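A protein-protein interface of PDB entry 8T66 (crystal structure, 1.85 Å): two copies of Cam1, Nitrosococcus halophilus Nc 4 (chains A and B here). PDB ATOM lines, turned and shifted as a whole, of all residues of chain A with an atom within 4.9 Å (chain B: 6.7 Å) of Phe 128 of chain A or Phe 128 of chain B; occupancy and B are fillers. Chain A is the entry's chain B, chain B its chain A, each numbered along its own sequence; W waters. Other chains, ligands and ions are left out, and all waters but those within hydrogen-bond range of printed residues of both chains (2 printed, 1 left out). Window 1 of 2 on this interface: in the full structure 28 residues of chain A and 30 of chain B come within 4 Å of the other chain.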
ATOM      1  N   PHE A  14       1.947  14.536 -11.076  1.00  0.00           N
ATOM      2  CA  PHE A  14       1.563  15.846 -11.596  1.00  0.00           C
ATOM      3  C   PHE A  14       2.662  16.307 -12.543  1.00  0.00           C
ATOM      4  O   PHE A  14       3.625  16.970 -12.130  1.00  0.00           O
ATOM      5  CB  PHE A  14       1.299  16.813 -10.448  1.00  0.00           C
ATOM      6  CG  PHE A  14       0.212  16.309  -9.516  1.00  0.00           C
ATOM      7  CD1 PHE A  14       0.526  15.463  -8.473  1.00  0.00           C
ATOM      8  CD2 PHE A  14      -1.124  16.623  -9.759  1.00  0.00           C
ATOM      9  CE1 PHE A  14      -0.482  14.949  -7.624  1.00  0.00           C
ATOM     10  CE2 PHE A  14      -2.141  16.118  -8.923  1.00  0.00           C
ATOM     11  CZ  PHE A  14      -1.807  15.272  -7.867  1.00  0.00           C
ATOM     12  N   LEU A 116      -9.399  27.992  -8.882  1.00  0.00           N
ATOM     13  CA  LEU A 116      -9.376  27.497  -7.500  1.00  0.00           C
ATOM     14  C   LEU A 116      -9.426  28.603  -6.463  1.00  0.00           C
ATOM     15  O   LEU A 116      -9.532  28.296  -5.266  1.00  0.00           O
ATOM     16  CB  LEU A 116      -8.087  26.694  -7.247  1.00  0.00           C
ATOM     17  CG  LEU A 116      -7.847  25.454  -8.083  1.00  0.00           C
ATOM     18  CD1 LEU A 116      -6.690  24.682  -7.520  1.00  0.00           C
ATOM     19  CD2 LEU A 116      -9.103  24.613  -8.059  1.00  0.00           C
ATOM     20  N   SER A 124     -11.514  24.543  -2.565  1.00  0.00           N
ATOM     21  CA  SER A 124     -10.536  24.598  -3.647  1.00  0.00           C
ATOM     22  C   SER A 124      -9.853  23.250  -3.856  1.00  0.00           C
ATOM     23  O   SER A 124      -9.620  22.836  -4.995  1.00  0.00           O
ATOM     24  CB  SER A 124      -9.500  25.672  -3.335  1.00  0.00           C
ATOM     25  OG  SER A 124     -10.125  26.922  -3.248  1.00  0.00           O
ATOM     26  N   LEU A 125      -9.540  22.534  -2.765  1.00  0.00           N
ATOM     27  CA  LEU A 125      -8.880  21.247  -2.940  1.00  0.00           C
ATOM     28  C   LEU A 125      -9.821  20.227  -3.570  1.00  0.00           C
ATOM     29  O   LEU A 125      -9.393  19.427  -4.406  1.00  0.00           O
ATOM     30  CB  LEU A 125      -8.338  20.741  -1.612  1.00  0.00           C
ATOM     31  CG  LEU A 125      -7.033  21.394  -1.149  1.00  0.00           C
ATOM     32  CD1 LEU A 125      -6.865  21.147   0.338  1.00  0.00           C
ATOM     33  CD2 LEU A 125      -5.860  20.800  -1.923  1.00  0.00           C
ATOM     34  N   GLY A 126     -11.100  20.229  -3.187  1.00  0.00           N
ATOM     35  CA  GLY A 126     -12.052  19.356  -3.875  1.00  0.00           C
ATOM     36  C   GLY A 126     -12.177  19.694  -5.353  1.00  0.00           C
ATOM     37  O   GLY A 126     -12.238  18.802  -6.202  1.00  0.00           O
ATOM     38  N   ALA A 127     -12.181  20.986  -5.677  1.00  0.00           N
ATOM     39  CA  ALA A 127     -12.250  21.415  -7.073  1.00  0.00           C
ATOM     40  C   ALA A 127     -11.016  20.973  -7.838  1.00  0.00           C
ATOM     41  O   ALA A 127     -11.112  20.544  -8.997  1.00  0.00           O
ATOM     42  CB  ALA A 127     -12.389  22.938  -7.155  1.00  0.00           C
ATOM     43  N   PHE A 128      -9.842  21.088  -7.211  1.00  0.00           N
ATOM     44  CA  PHE A 128      -8.612  20.614  -7.840  1.00  0.00           C
ATOM     45  C   PHE A 128      -8.699  19.123  -8.144  1.00  0.00           C
ATOM     46  O   PHE A 128      -8.319  18.678  -9.233  1.00  0.00           O
ATOM     47  CB  PHE A 128      -7.412  20.916  -6.934  1.00  0.00           C
ATOM     48  CG  PHE A 128      -6.093  20.400  -7.464  1.00  0.00           C
ATOM     49  CD1 PHE A 128      -5.456  21.040  -8.526  1.00  0.00           C
ATOM     50  CD2 PHE A 128      -5.488  19.290  -6.891  1.00  0.00           C
ATOM     51  CE1 PHE A 128      -4.230  20.575  -9.006  1.00  0.00           C
ATOM     52  CE2 PHE A 128      -4.269  18.807  -7.371  1.00  0.00           C
ATOM     53  CZ  PHE A 128      -3.634  19.465  -8.438  1.00  0.00           C
ATOM     54  N   MET A 129      -9.193  18.326  -7.188  1.00  0.00           N
ATOM     55  CA  MET A 129      -9.240  16.884  -7.413  1.00  0.00           C
ATOM     56  C   MET A 129     -10.200  16.538  -8.548  1.00  0.00           C
ATOM     57  O   MET A 129      -9.928  15.638  -9.354  1.00  0.00           O
ATOM     58  CB  MET A 129      -9.627  16.163  -6.120  1.00  0.00           C
ATOM     59  CG  MET A 129      -8.488  16.122  -5.093  1.00  0.00           C
ATOM     60  SD  MET A 129      -8.943  15.174  -3.600  1.00  0.00           S
ATOM     61  CE  MET A 129      -9.390  16.502  -2.495  1.00  0.00           C
ATOM     62  N   ALA A 130     -11.320  17.253  -8.640  1.00  0.00           N
ATOM     63  CA  ALA A 130     -12.251  17.034  -9.749  1.00  0.00           C
ATOM     64  C   ALA A 130     -11.628  17.458 -11.072  1.00  0.00           C
ATOM     65  O   ALA A 130     -11.808  16.795 -12.107  1.00  0.00           O
ATOM     66  CB  ALA A 130     -13.543  17.818  -9.501  1.00  0.00           C
ATOM     67  N   ALA A 131     -10.908  18.577 -11.066  1.00  0.00           N
ATOM     68  CA  ALA A 131     -10.251  19.008 -12.298  1.00  0.00           C
ATOM     69  C   ALA A 131      -9.256  17.955 -12.764  1.00  0.00           C
ATOM     70  O   ALA A 131      -9.255  17.556 -13.938  1.00  0.00           O
ATOM     71  CB  ALA A 131      -9.571  20.363 -12.086  1.00  0.00           C
ATOM     72  N   GLU A 132      -8.431  17.454 -11.839  1.00  0.00           N
ATOM     73  CA  GLU A 132      -7.430  16.446 -12.182  1.00  0.00           C
ATOM     74  C   GLU A 132      -8.073  15.177 -12.727  1.00  0.00           C
ATOM     75  O   GLU A 132      -7.584  14.584 -13.699  1.00  0.00           O
ATOM     76  CB  GLU A 132      -6.578  16.124 -10.954  1.00  0.00           C
ATOM     77  CG  GLU A 132      -5.574  17.217 -10.612  1.00  0.00           C
ATOM     78  CD  GLU A 132      -4.450  17.305 -11.634  1.00  0.00           C
ATOM     79  OE1 GLU A 132      -4.093  18.427 -12.092  1.00  0.00           O
ATOM     80  OE2 GLU A 132      -3.917  16.228 -11.987  1.00  0.00           O
ATOM     81  N   SER A 138      -6.080  23.589 -13.770  1.00  0.00           N
ATOM     82  CA  SER A 138      -6.478  24.382 -12.615  1.00  0.00           C
ATOM     83  C   SER A 138      -5.679  25.679 -12.579  1.00  0.00           C
ATOM     84  O   SER A 138      -4.476  25.693 -12.857  1.00  0.00           O
ATOM     85  CB  SER A 138      -6.271  23.613 -11.313  1.00  0.00           C
ATOM     86  OG  SER A 138      -5.083  22.838 -11.396  1.00  0.00           O
ATOM     87  N   ILE A 162      -1.913  26.057 -11.839  1.00  0.00           N
ATOM     88  CA  ILE A 162      -1.585  25.127 -10.760  1.00  0.00           C
ATOM     89  C   ILE A 162      -1.056  23.828 -11.346  1.00  0.00           C
ATOM     90  O   ILE A 162       0.092  23.439 -11.102  1.00  0.00           O
ATOM     91  CB  ILE A 162      -2.801  24.892  -9.840  1.00  0.00           C
ATOM     92  CG1 ILE A 162      -3.231  26.201  -9.193  1.00  0.00           C
ATOM     93  CG2 ILE A 162      -2.426  23.895  -8.746  1.00  0.00           C
ATOM     94  CD1 ILE A 162      -2.097  26.885  -8.399  1.00  0.00           C
ATOM     95  N   SER A 163      -1.876  23.171 -12.153  1.00  0.00           N
ATOM     96  CA  SER A 163      -1.533  21.897 -12.759  1.00  0.00           C
ATOM     97  C   SER A 163      -2.169  21.857 -14.139  1.00  0.00           C
ATOM     98  O   SER A 163      -3.211  22.474 -14.355  1.00  0.00           O
ATOM     99  CB  SER A 163      -2.019  20.725 -11.900  1.00  0.00           C
ATOM    100  OG  SER A 163      -1.907  19.511 -12.605  1.00  0.00           O
ATOM    101  N   ASN B  12      -5.109  11.276 -12.824  1.00  0.00           N
ATOM    102  CA  ASN B  12      -5.035  11.022 -11.401  1.00  0.00           C
ATOM    103  C   ASN B  12      -6.415  10.652 -10.868  1.00  0.00           C
ATOM    104  O   ASN B  12      -7.450  10.977 -11.463  1.00  0.00           O
ATOM    105  CB  ASN B  12      -4.449  12.249 -10.700  1.00  0.00           C
ATOM    106  CG  ASN B  12      -2.995  12.456 -11.076  1.00  0.00           C
ATOM    107  OD1 ASN B  12      -2.275  11.482 -11.269  1.00  0.00           O
ATOM    108  ND2 ASN B  12      -2.566  13.710 -11.226  1.00  0.00           N
ATOM    109  N   PHE B  14      -8.557  10.009  -6.925  1.00  0.00           N
ATOM    110  CA  PHE B  14      -8.551  10.267  -5.485  1.00  0.00           C
ATOM    111  C   PHE B  14      -9.603   9.376  -4.836  1.00  0.00           C
ATOM    112  O   PHE B  14     -10.761   9.779  -4.666  1.00  0.00           O
ATOM    113  CB  PHE B  14      -8.777  11.756  -5.224  1.00  0.00           C
ATOM    114  CG  PHE B  14      -7.767  12.616  -5.950  1.00  0.00           C
ATOM    115  CD1 PHE B  14      -6.527  12.871  -5.378  1.00  0.00           C
ATOM    116  CD2 PHE B  14      -8.013  13.067  -7.235  1.00  0.00           C
ATOM    117  CE1 PHE B  14      -5.563  13.623  -6.070  1.00  0.00           C
ATOM    118  CE2 PHE B  14      -7.055  13.820  -7.934  1.00  0.00           C
ATOM    119  CZ  PHE B  14      -5.822  14.086  -7.341  1.00  0.00           C
ATOM    120  N   ARG B  94       5.777  22.324  -3.858  1.00  0.00           N
ATOM    121  CA  ARG B  94       5.818  20.900  -4.166  1.00  0.00           C
ATOM    122  C   ARG B  94       7.220  20.335  -3.979  1.00  0.00           C
ATOM    123  O   ARG B  94       7.401  19.285  -3.360  1.00  0.00           O
ATOM    124  CB  ARG B  94       5.330  20.654  -5.603  1.00  0.00           C
ATOM    125  CG  ARG B  94       4.894  19.207  -5.925  1.00  0.00           C
ATOM    126  CD  ARG B  94       5.897  18.408  -6.774  1.00  0.00           C
ATOM    127  NE  ARG B  94       6.195  19.097  -8.019  1.00  0.00           N
ATOM    128  CZ  ARG B  94       5.903  18.629  -9.224  1.00  0.00           C
ATOM    129  NH1 ARG B  94       5.304  17.447  -9.369  1.00  0.00           N
ATOM    130  NH2 ARG B  94       6.227  19.344 -10.277  1.00  0.00           N
ATOM    131  N   VAL B  97       8.322  20.420  -0.138  1.00  0.00           N
ATOM    132  CA  VAL B  97       7.615  19.434   0.677  1.00  0.00           C
ATOM    133  C   VAL B  97       8.067  18.024   0.320  1.00  0.00           C
ATOM    134  O   VAL B  97       8.271  17.188   1.205  1.00  0.00           O
ATOM    135  CB  VAL B  97       6.085  19.598   0.550  1.00  0.00           C
ATOM    136  CG1 VAL B  97       5.355  18.386   1.189  1.00  0.00           C
ATOM    137  CG2 VAL B  97       5.644  20.895   1.256  1.00  0.00           C
ATOM    138  N   VAL B 114       0.899  15.439   5.695  1.00  0.00           N
ATOM    139  CA  VAL B 114       1.185  16.811   5.293  1.00  0.00           C
ATOM    140  C   VAL B 114       0.008  17.666   5.742  1.00  0.00           C
ATOM    141  O   VAL B 114      -1.130  17.430   5.318  1.00  0.00           O
ATOM    142  CB  VAL B 114       1.401  16.913   3.777  1.00  0.00           C
ATOM    143  CG1 VAL B 114       1.455  18.372   3.360  1.00  0.00           C
ATOM    144  CG2 VAL B 114       2.673  16.153   3.364  1.00  0.00           C
ATOM    145  N   LEU B 116      -1.497  20.992   5.162  1.00  0.00           N
ATOM    146  CA  LEU B 116      -1.367  22.038   4.158  1.00  0.00           C
ATOM    147  C   LEU B 116      -2.176  23.288   4.504  1.00  0.00           C
ATOM    148  O   LEU B 116      -2.399  24.132   3.628  1.00  0.00           O
ATOM    149  CB  LEU B 116      -1.754  21.479   2.783  1.00  0.00           C
ATOM    150  CG  LEU B 116      -2.976  20.543   2.750  1.00  0.00           C
ATOM    151  CD1 LEU B 116      -4.241  21.290   3.067  1.00  0.00           C
ATOM    152  CD2 LEU B 116      -3.121  19.899   1.373  1.00  0.00           C
ATOM    153  N   MET B 123       0.990  27.379  -2.149  1.00  0.00           N
ATOM    154  CA  MET B 123       1.814  26.595  -1.232  1.00  0.00           C
ATOM    155  C   MET B 123       1.072  25.340  -0.793  1.00  0.00           C
ATOM    156  O   MET B 123       1.629  24.233  -0.806  1.00  0.00           O
ATOM    157  CB  MET B 123       2.215  27.441  -0.021  1.00  0.00           C
ATOM    158  CG  MET B 123       3.089  28.652  -0.391  1.00  0.00           C
ATOM    159  SD  MET B 123       3.268  29.771   1.012  1.00  0.00           S
ATOM    160  CE  MET B 123       4.021  28.649   2.208  1.00  0.00           C
ATOM    161  N   SER B 124      -0.189  25.498  -0.410  1.00  0.00           N
ATOM    162  CA  SER B 124      -1.005  24.366   0.012  1.00  0.00           C
ATOM    163  C   SER B 124      -1.211  23.364  -1.122  1.00  0.00           C
ATOM    164  O   SER B 124      -1.211  22.148  -0.887  1.00  0.00           O
ATOM    165  CB  SER B 124      -2.355  24.871   0.508  1.00  0.00           C
ATOM    166  OG  SER B 124      -2.221  25.756   1.600  1.00  0.00           O
ATOM    167  N   LEU B 125      -1.414  23.853  -2.353  1.00  0.00           N
ATOM    168  CA  LEU B 125      -1.647  22.944  -3.477  1.00  0.00           C
ATOM    169  C   LEU B 125      -0.365  22.218  -3.868  1.00  0.00           C
ATOM    170  O   LEU B 125      -0.400  21.050  -4.256  1.00  0.00           O
ATOM    171  CB  LEU B 125      -2.225  23.715  -4.666  1.00  0.00           C
ATOM    172  CG  LEU B 125      -3.768  23.704  -4.815  1.00  0.00           C
ATOM    173  CD1 LEU B 125      -4.226  22.357  -5.331  1.00  0.00           C
ATOM    174  CD2 LEU B 125      -4.481  24.033  -3.514  1.00  0.00           C
ATOM    175  N   GLY B 126       0.783  22.891  -3.779  1.00  0.00           N
ATOM    176  CA  GLY B 126       2.037  22.195  -4.024  1.00  0.00           C
ATOM    177  C   GLY B 126       2.299  21.131  -2.976  1.00  0.00           C
ATOM    178  O   GLY B 126       2.714  20.015  -3.300  1.00  0.00           O
ATOM    179  N   ALA B 127       2.052  21.463  -1.708  1.00  0.00           N
ATOM    180  CA  ALA B 127       2.147  20.483  -0.626  1.00  0.00           C
ATOM    181  C   ALA B 127       1.232  19.286  -0.874  1.00  0.00           C
ATOM    182  O   ALA B 127       1.628  18.130  -0.670  1.00  0.00           O
ATOM    183  CB  ALA B 127       1.800  21.163   0.695  1.00  0.00           C
ATOM    184  N   PHE B 128       0.010  19.544  -1.337  1.00  0.00           N
ATOM    185  CA  PHE B 128      -0.922  18.456  -1.631  1.00  0.00           C
ATOM    186  C   PHE B 128      -0.377  17.541  -2.723  1.00  0.00           C
ATOM    187  O   PHE B 128      -0.447  16.305  -2.614  1.00  0.00           O
ATOM    188  CB  PHE B 128      -2.275  19.034  -2.055  1.00  0.00           C
ATOM    189  CG  PHE B 128      -3.266  17.981  -2.480  1.00  0.00           C
ATOM    190  CD1 PHE B 128      -3.854  17.158  -1.529  1.00  0.00           C
ATOM    191  CD2 PHE B 128      -3.594  17.811  -3.821  1.00  0.00           C
ATOM    192  CE1 PHE B 128      -4.771  16.174  -1.911  1.00  0.00           C
ATOM    193  CE2 PHE B 128      -4.506  16.841  -4.218  1.00  0.00           C
ATOM    194  CZ  PHE B 128      -5.097  16.010  -3.251  1.00  0.00           C
ATOM    195  N   MET B 129       0.143  18.132  -3.809  1.00  0.00           N
ATOM    196  CA  MET B 129       0.677  17.317  -4.896  1.00  0.00           C
ATOM    197  C   MET B 129       1.860  16.485  -4.426  1.00  0.00           C
ATOM    198  O   MET B 129       1.986  15.309  -4.788  1.00  0.00           O
ATOM    199  CB  MET B 129       1.061  18.206  -6.077  1.00  0.00           C
ATOM    200  CG  MET B 129      -0.165  18.817  -6.766  1.00  0.00           C
ATOM    201  SD  MET B 129       0.254  19.730  -8.281  1.00  0.00           S
ATOM    202  CE  MET B 129       0.728  21.281  -7.564  1.00  0.00           C
ATOM    203  N   ALA B 130       2.730  17.072  -3.608  1.00  0.00           N
ATOM    204  CA  ALA B 130       3.856  16.319  -3.063  1.00  0.00           C
ATOM    205  C   ALA B 130       3.377  15.199  -2.150  1.00  0.00           C
ATOM    206  O   ALA B 130       3.959  14.104  -2.135  1.00  0.00           O
ATOM    207  CB  ALA B 130       4.783  17.253  -2.287  1.00  0.00           C
ATOM    208  N   ALA B 131       2.353  15.476  -1.344  1.00  0.00           N
ATOM    209  CA  ALA B 131       1.780  14.428  -0.502  1.00  0.00           C
ATOM    210  C   ALA B 131       1.261  13.281  -1.356  1.00  0.00           C
ATOM    211  O   ALA B 131       1.589  12.113  -1.115  1.00  0.00           O
ATOM    212  CB  ALA B 131       0.666  15.015   0.372  1.00  0.00           C
ATOM    213  N   GLU B 132       0.470  13.605  -2.386  1.00  0.00           N
ATOM    214  CA  GLU B 132      -0.097  12.580  -3.258  1.00  0.00           C
ATOM    215  C   GLU B 132       0.987  11.774  -3.960  1.00  0.00           C
ATOM    216  O   GLU B 132       0.871  10.549  -4.099  1.00  0.00           O
ATOM    217  CB  GLU B 132      -1.020  13.235  -4.294  1.00  0.00           C
ATOM    218  CG  GLU B 132      -2.345  13.682  -3.698  1.00  0.00           C
ATOM    219  CD  GLU B 132      -3.219  12.493  -3.352  1.00  0.00           C
ATOM    220  OE1 GLU B 132      -3.383  11.599  -4.229  1.00  0.00           O
ATOM    221  OE2 GLU B 132      -3.722  12.440  -2.198  1.00  0.00           O
ATOM    222  N   GLU B 133       2.041  12.446  -4.442  1.00  0.00           N
ATOM    223  CA  GLU B 133       3.095  11.726  -5.151  1.00  0.00           C
ATOM    224  C   GLU B 133       3.870  10.786  -4.236  1.00  0.00           C
ATOM    225  O   GLU B 133       4.362   9.751  -4.697  1.00  0.00           O
ATOM    226  CB  GLU B 133       4.037  12.726  -5.834  1.00  0.00           C
ATOM    227  CG  GLU B 133       3.368  13.365  -7.026  1.00  0.00           C
ATOM    228  CD  GLU B 133       4.287  14.304  -7.776  1.00  0.00           C
ATOM    229  OE1 GLU B 133       5.217  14.847  -7.135  1.00  0.00           O
ATOM    230  OE2 GLU B 133       4.042  14.503  -8.988  1.00  0.00           O
ATOM    231  N   VAL B 136       1.252   9.882   0.806  1.00  0.00           N
ATOM    232  CA  VAL B 136       0.980  10.230   2.195  1.00  0.00           C
ATOM    233  C   VAL B 136      -0.274  11.094   2.286  1.00  0.00           C
ATOM    234  O   VAL B 136      -0.649  11.810   1.347  1.00  0.00           O
ATOM    235  CB  VAL B 136       2.180  10.918   2.885  1.00  0.00           C
ATOM    236  CG1 VAL B 136       3.483  10.210   2.546  1.00  0.00           C
ATOM    237  CG2 VAL B 136       2.265  12.354   2.522  1.00  0.00           C
ATOM    238  N   SER B 138      -2.994  13.962   3.357  1.00  0.00           N
ATOM    239  CA  SER B 138      -2.998  15.412   3.499  1.00  0.00           C
ATOM    240  C   SER B 138      -4.093  15.832   4.471  1.00  0.00           C
ATOM    241  O   SER B 138      -5.196  15.273   4.456  1.00  0.00           O
ATOM    242  CB  SER B 138      -3.194  16.119   2.143  1.00  0.00           C
ATOM    243  OG  SER B 138      -4.152  15.461   1.319  1.00  0.00           O
ATOM    244  N   ILE B 162      -8.020  15.684   3.798  1.00  0.00           N
ATOM    245  CA  ILE B 162      -8.268  16.021   2.395  1.00  0.00           C
ATOM    246  C   ILE B 162      -8.276  14.761   1.542  1.00  0.00           C
ATOM    247  O   ILE B 162      -9.270  14.459   0.871  1.00  0.00           O
ATOM    248  CB  ILE B 162      -7.230  17.037   1.888  1.00  0.00           C
ATOM    249  CG1 ILE B 162      -7.256  18.280   2.774  1.00  0.00           C
ATOM    250  CG2 ILE B 162      -7.515  17.387   0.412  1.00  0.00           C
ATOM    251  CD1 ILE B 162      -8.630  19.003   2.813  1.00  0.00           C
ATOM    252  N   SER B 163      -7.176  14.007   1.563  1.00  0.00           N
ATOM    253  CA  SER B 163      -7.057  12.803   0.748  1.00  0.00           C
ATOM    254  C   SER B 163      -6.176  11.786   1.469  1.00  0.00           C
ATOM    255  O   SER B 163      -5.207  12.156   2.139  1.00  0.00           O
ATOM    256  CB  SER B 163      -6.466  13.134  -0.642  1.00  0.00           C
ATOM    257  OG  SER B 163      -6.264  11.953  -1.413  1.00  0.00           O
HETATM  258  O   HOH W   1      -4.933  14.131 -13.863  1.00  0.00           O
HETATM  259  O   HOH W   2      -1.676  16.209 -13.414  1.00  0.00           O
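Of the 14 printed residues of chain A, 5 touch a printed residue of chain B.
Hydrophobic or aromatic side chains of chain A within 4 Å of the printed part of chain B: Phe 14, Leu 125, Phe 128 and Met 129.
Of the 21 printed residues of chain B, 10 touch a printed residue of chain A.
Hydrophobic or aromatic side chains of chain B that line the printed part of chain A: Phe 14, Leu 116, Leu 125, Phe 128, Met 129 and Ile 162.
Among the printed residues, 17 pairs touch across the chains.
Among the printed residues, no Asp or Glu carboxylate lies within 4 Å of a Lys or Arg side-chain nitrogen of the other chain.
Asn 12 of chain B touches Phe 14 of chain A (ND2 to CE2, 3.4 Å).
CG of Phe 14 of chain A touches SD of Met 129 of chain B, at 3.6 Å.
Leu 125 of chain A touches Leu 125 of chain B (CD2 to CD2, 3.9 Å).
Leu 125 of chain A touches Phe 128 of chain B (CD2 to CG, 3.9 Å).
CD1 of Ile 162 of chain B touches CD1 of Leu 125 of chain A, 3.7 Å away.
CG of Phe 128 of chain A touches CD1 of Leu 125 of chain B (3.4 Å).
CE2 of Phe 128 of chain A touches CE2 of Phe 128 of chain B, 3.7 Å away.
Phe 128 of chain A touches Met 129 of chain B.
Phe 14 of chain B touches Met 129 of chain A (CD2 to CB, 3.7 Å).
Glu 132 of chain A touches Phe 14 of chain B.
The side-chain carboxylate (OE2) of Glu 133 of chain B sits at hydrogen-bond distance from the backbone NH (N) of Phe 14 of chain A.
ND2 of Asn 12 of chain B sits at hydrogen-bond distance from OE2 of Glu 132 of chain A, 3.0 Å away.
O of Phe 14 of chain A is in hydrogen-bond range of NH1 of Arg 94 of chain B (3.3 Å).
Water W2 lies within hydrogen-bond range of OE2 of Glu 132 of chain A (2.7 Å), OG of Ser 163 of chain A (3.4 Å) and ND2 of Asn 12 of chain B (3.4 Å).
Water W1 lies within hydrogen-bond range of the backbone carbonyl oxygen of Glu 132 of chain A and the backbone NH of Asn 12 of chain B.
The backbone NH of Ile 162 of chain B is in hydrogen-bond range of the backbone carbonyl oxygen of Ser 138 of chain B (2.9 Å).
OE1 of Glu 132 of chain A sits at hydrogen-bond distance from OG of Ser 163 of chain A (2.5 Å).
O of Leu 116 of chain B lies within hydrogen-bond range of OG of Ser 124 of chain B.
OE2 of Glu 132 of chain B sits at hydrogen-bond distance from OG of Ser 163 of chain B, 2.7 Å away.
NH1 of Arg 94 of chain B is in salt-bridge range of OE2 of Glu 133 of chain B (3.2 Å).
Phe 14 of chain A touches Met 129 of chain B, and with the chains exchanged Met 129 of chain A touches Phe 14 of chain B.
Leu 125 of chain A touches Leu 116 of chain B, but with the chains exchanged Leu 116 of chain A does not touch Leu 125 of chain B (4.03 Å).
Leu 125 of chain A touches Phe 128 of chain B, and with the chains exchanged Phe 128 of chain A touches Leu 125 of chain B.
Phe 128 of chain A touches Met 129 of chain B, and with the chains exchanged Met 129 of chain A touches Phe 128 of chain B.
Positions printed for both chains: 14, 116, 124, 125, 126, 127, 128, 129, 130, 131, 132, 138, 162 and 163.
Of the 17 pairs that touch across the chains among the printed residues, 10 have their exchanged pair printed and touching as well.
Printed residues of chain B within 4 Å of Phe 128 of chain A: Leu 125, Phe 128 and Met 129.
Phe 128 of chain B touches just these residues of chain A: Leu 125, Phe 128 and Met 129.
Printed residues of chain A within 4 Å of Phe 14 of chain B: Met 129 and Glu 132.
Printed residues of chain A within 4 Å of Glu 133 of chain B: Phe 14 (3.0 Å).
Of the printed residues of chain A, Asn 12 of chain B touches Phe 14 (3.4 Å) and Glu 132 (3.0 Å).
Of the printed residues of chain A, Leu 116 of chain B touches Leu 125.
Of the printed residues of chain B, Glu 132 of chain A touches Asn 12 and Phe 14.
Ser 124 of chain A touches none of the printed residues of chain B.
The nearest residue of chain A that does not touch Phe 128 of chain B is Phe 14 of chain A (4.8 Å).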
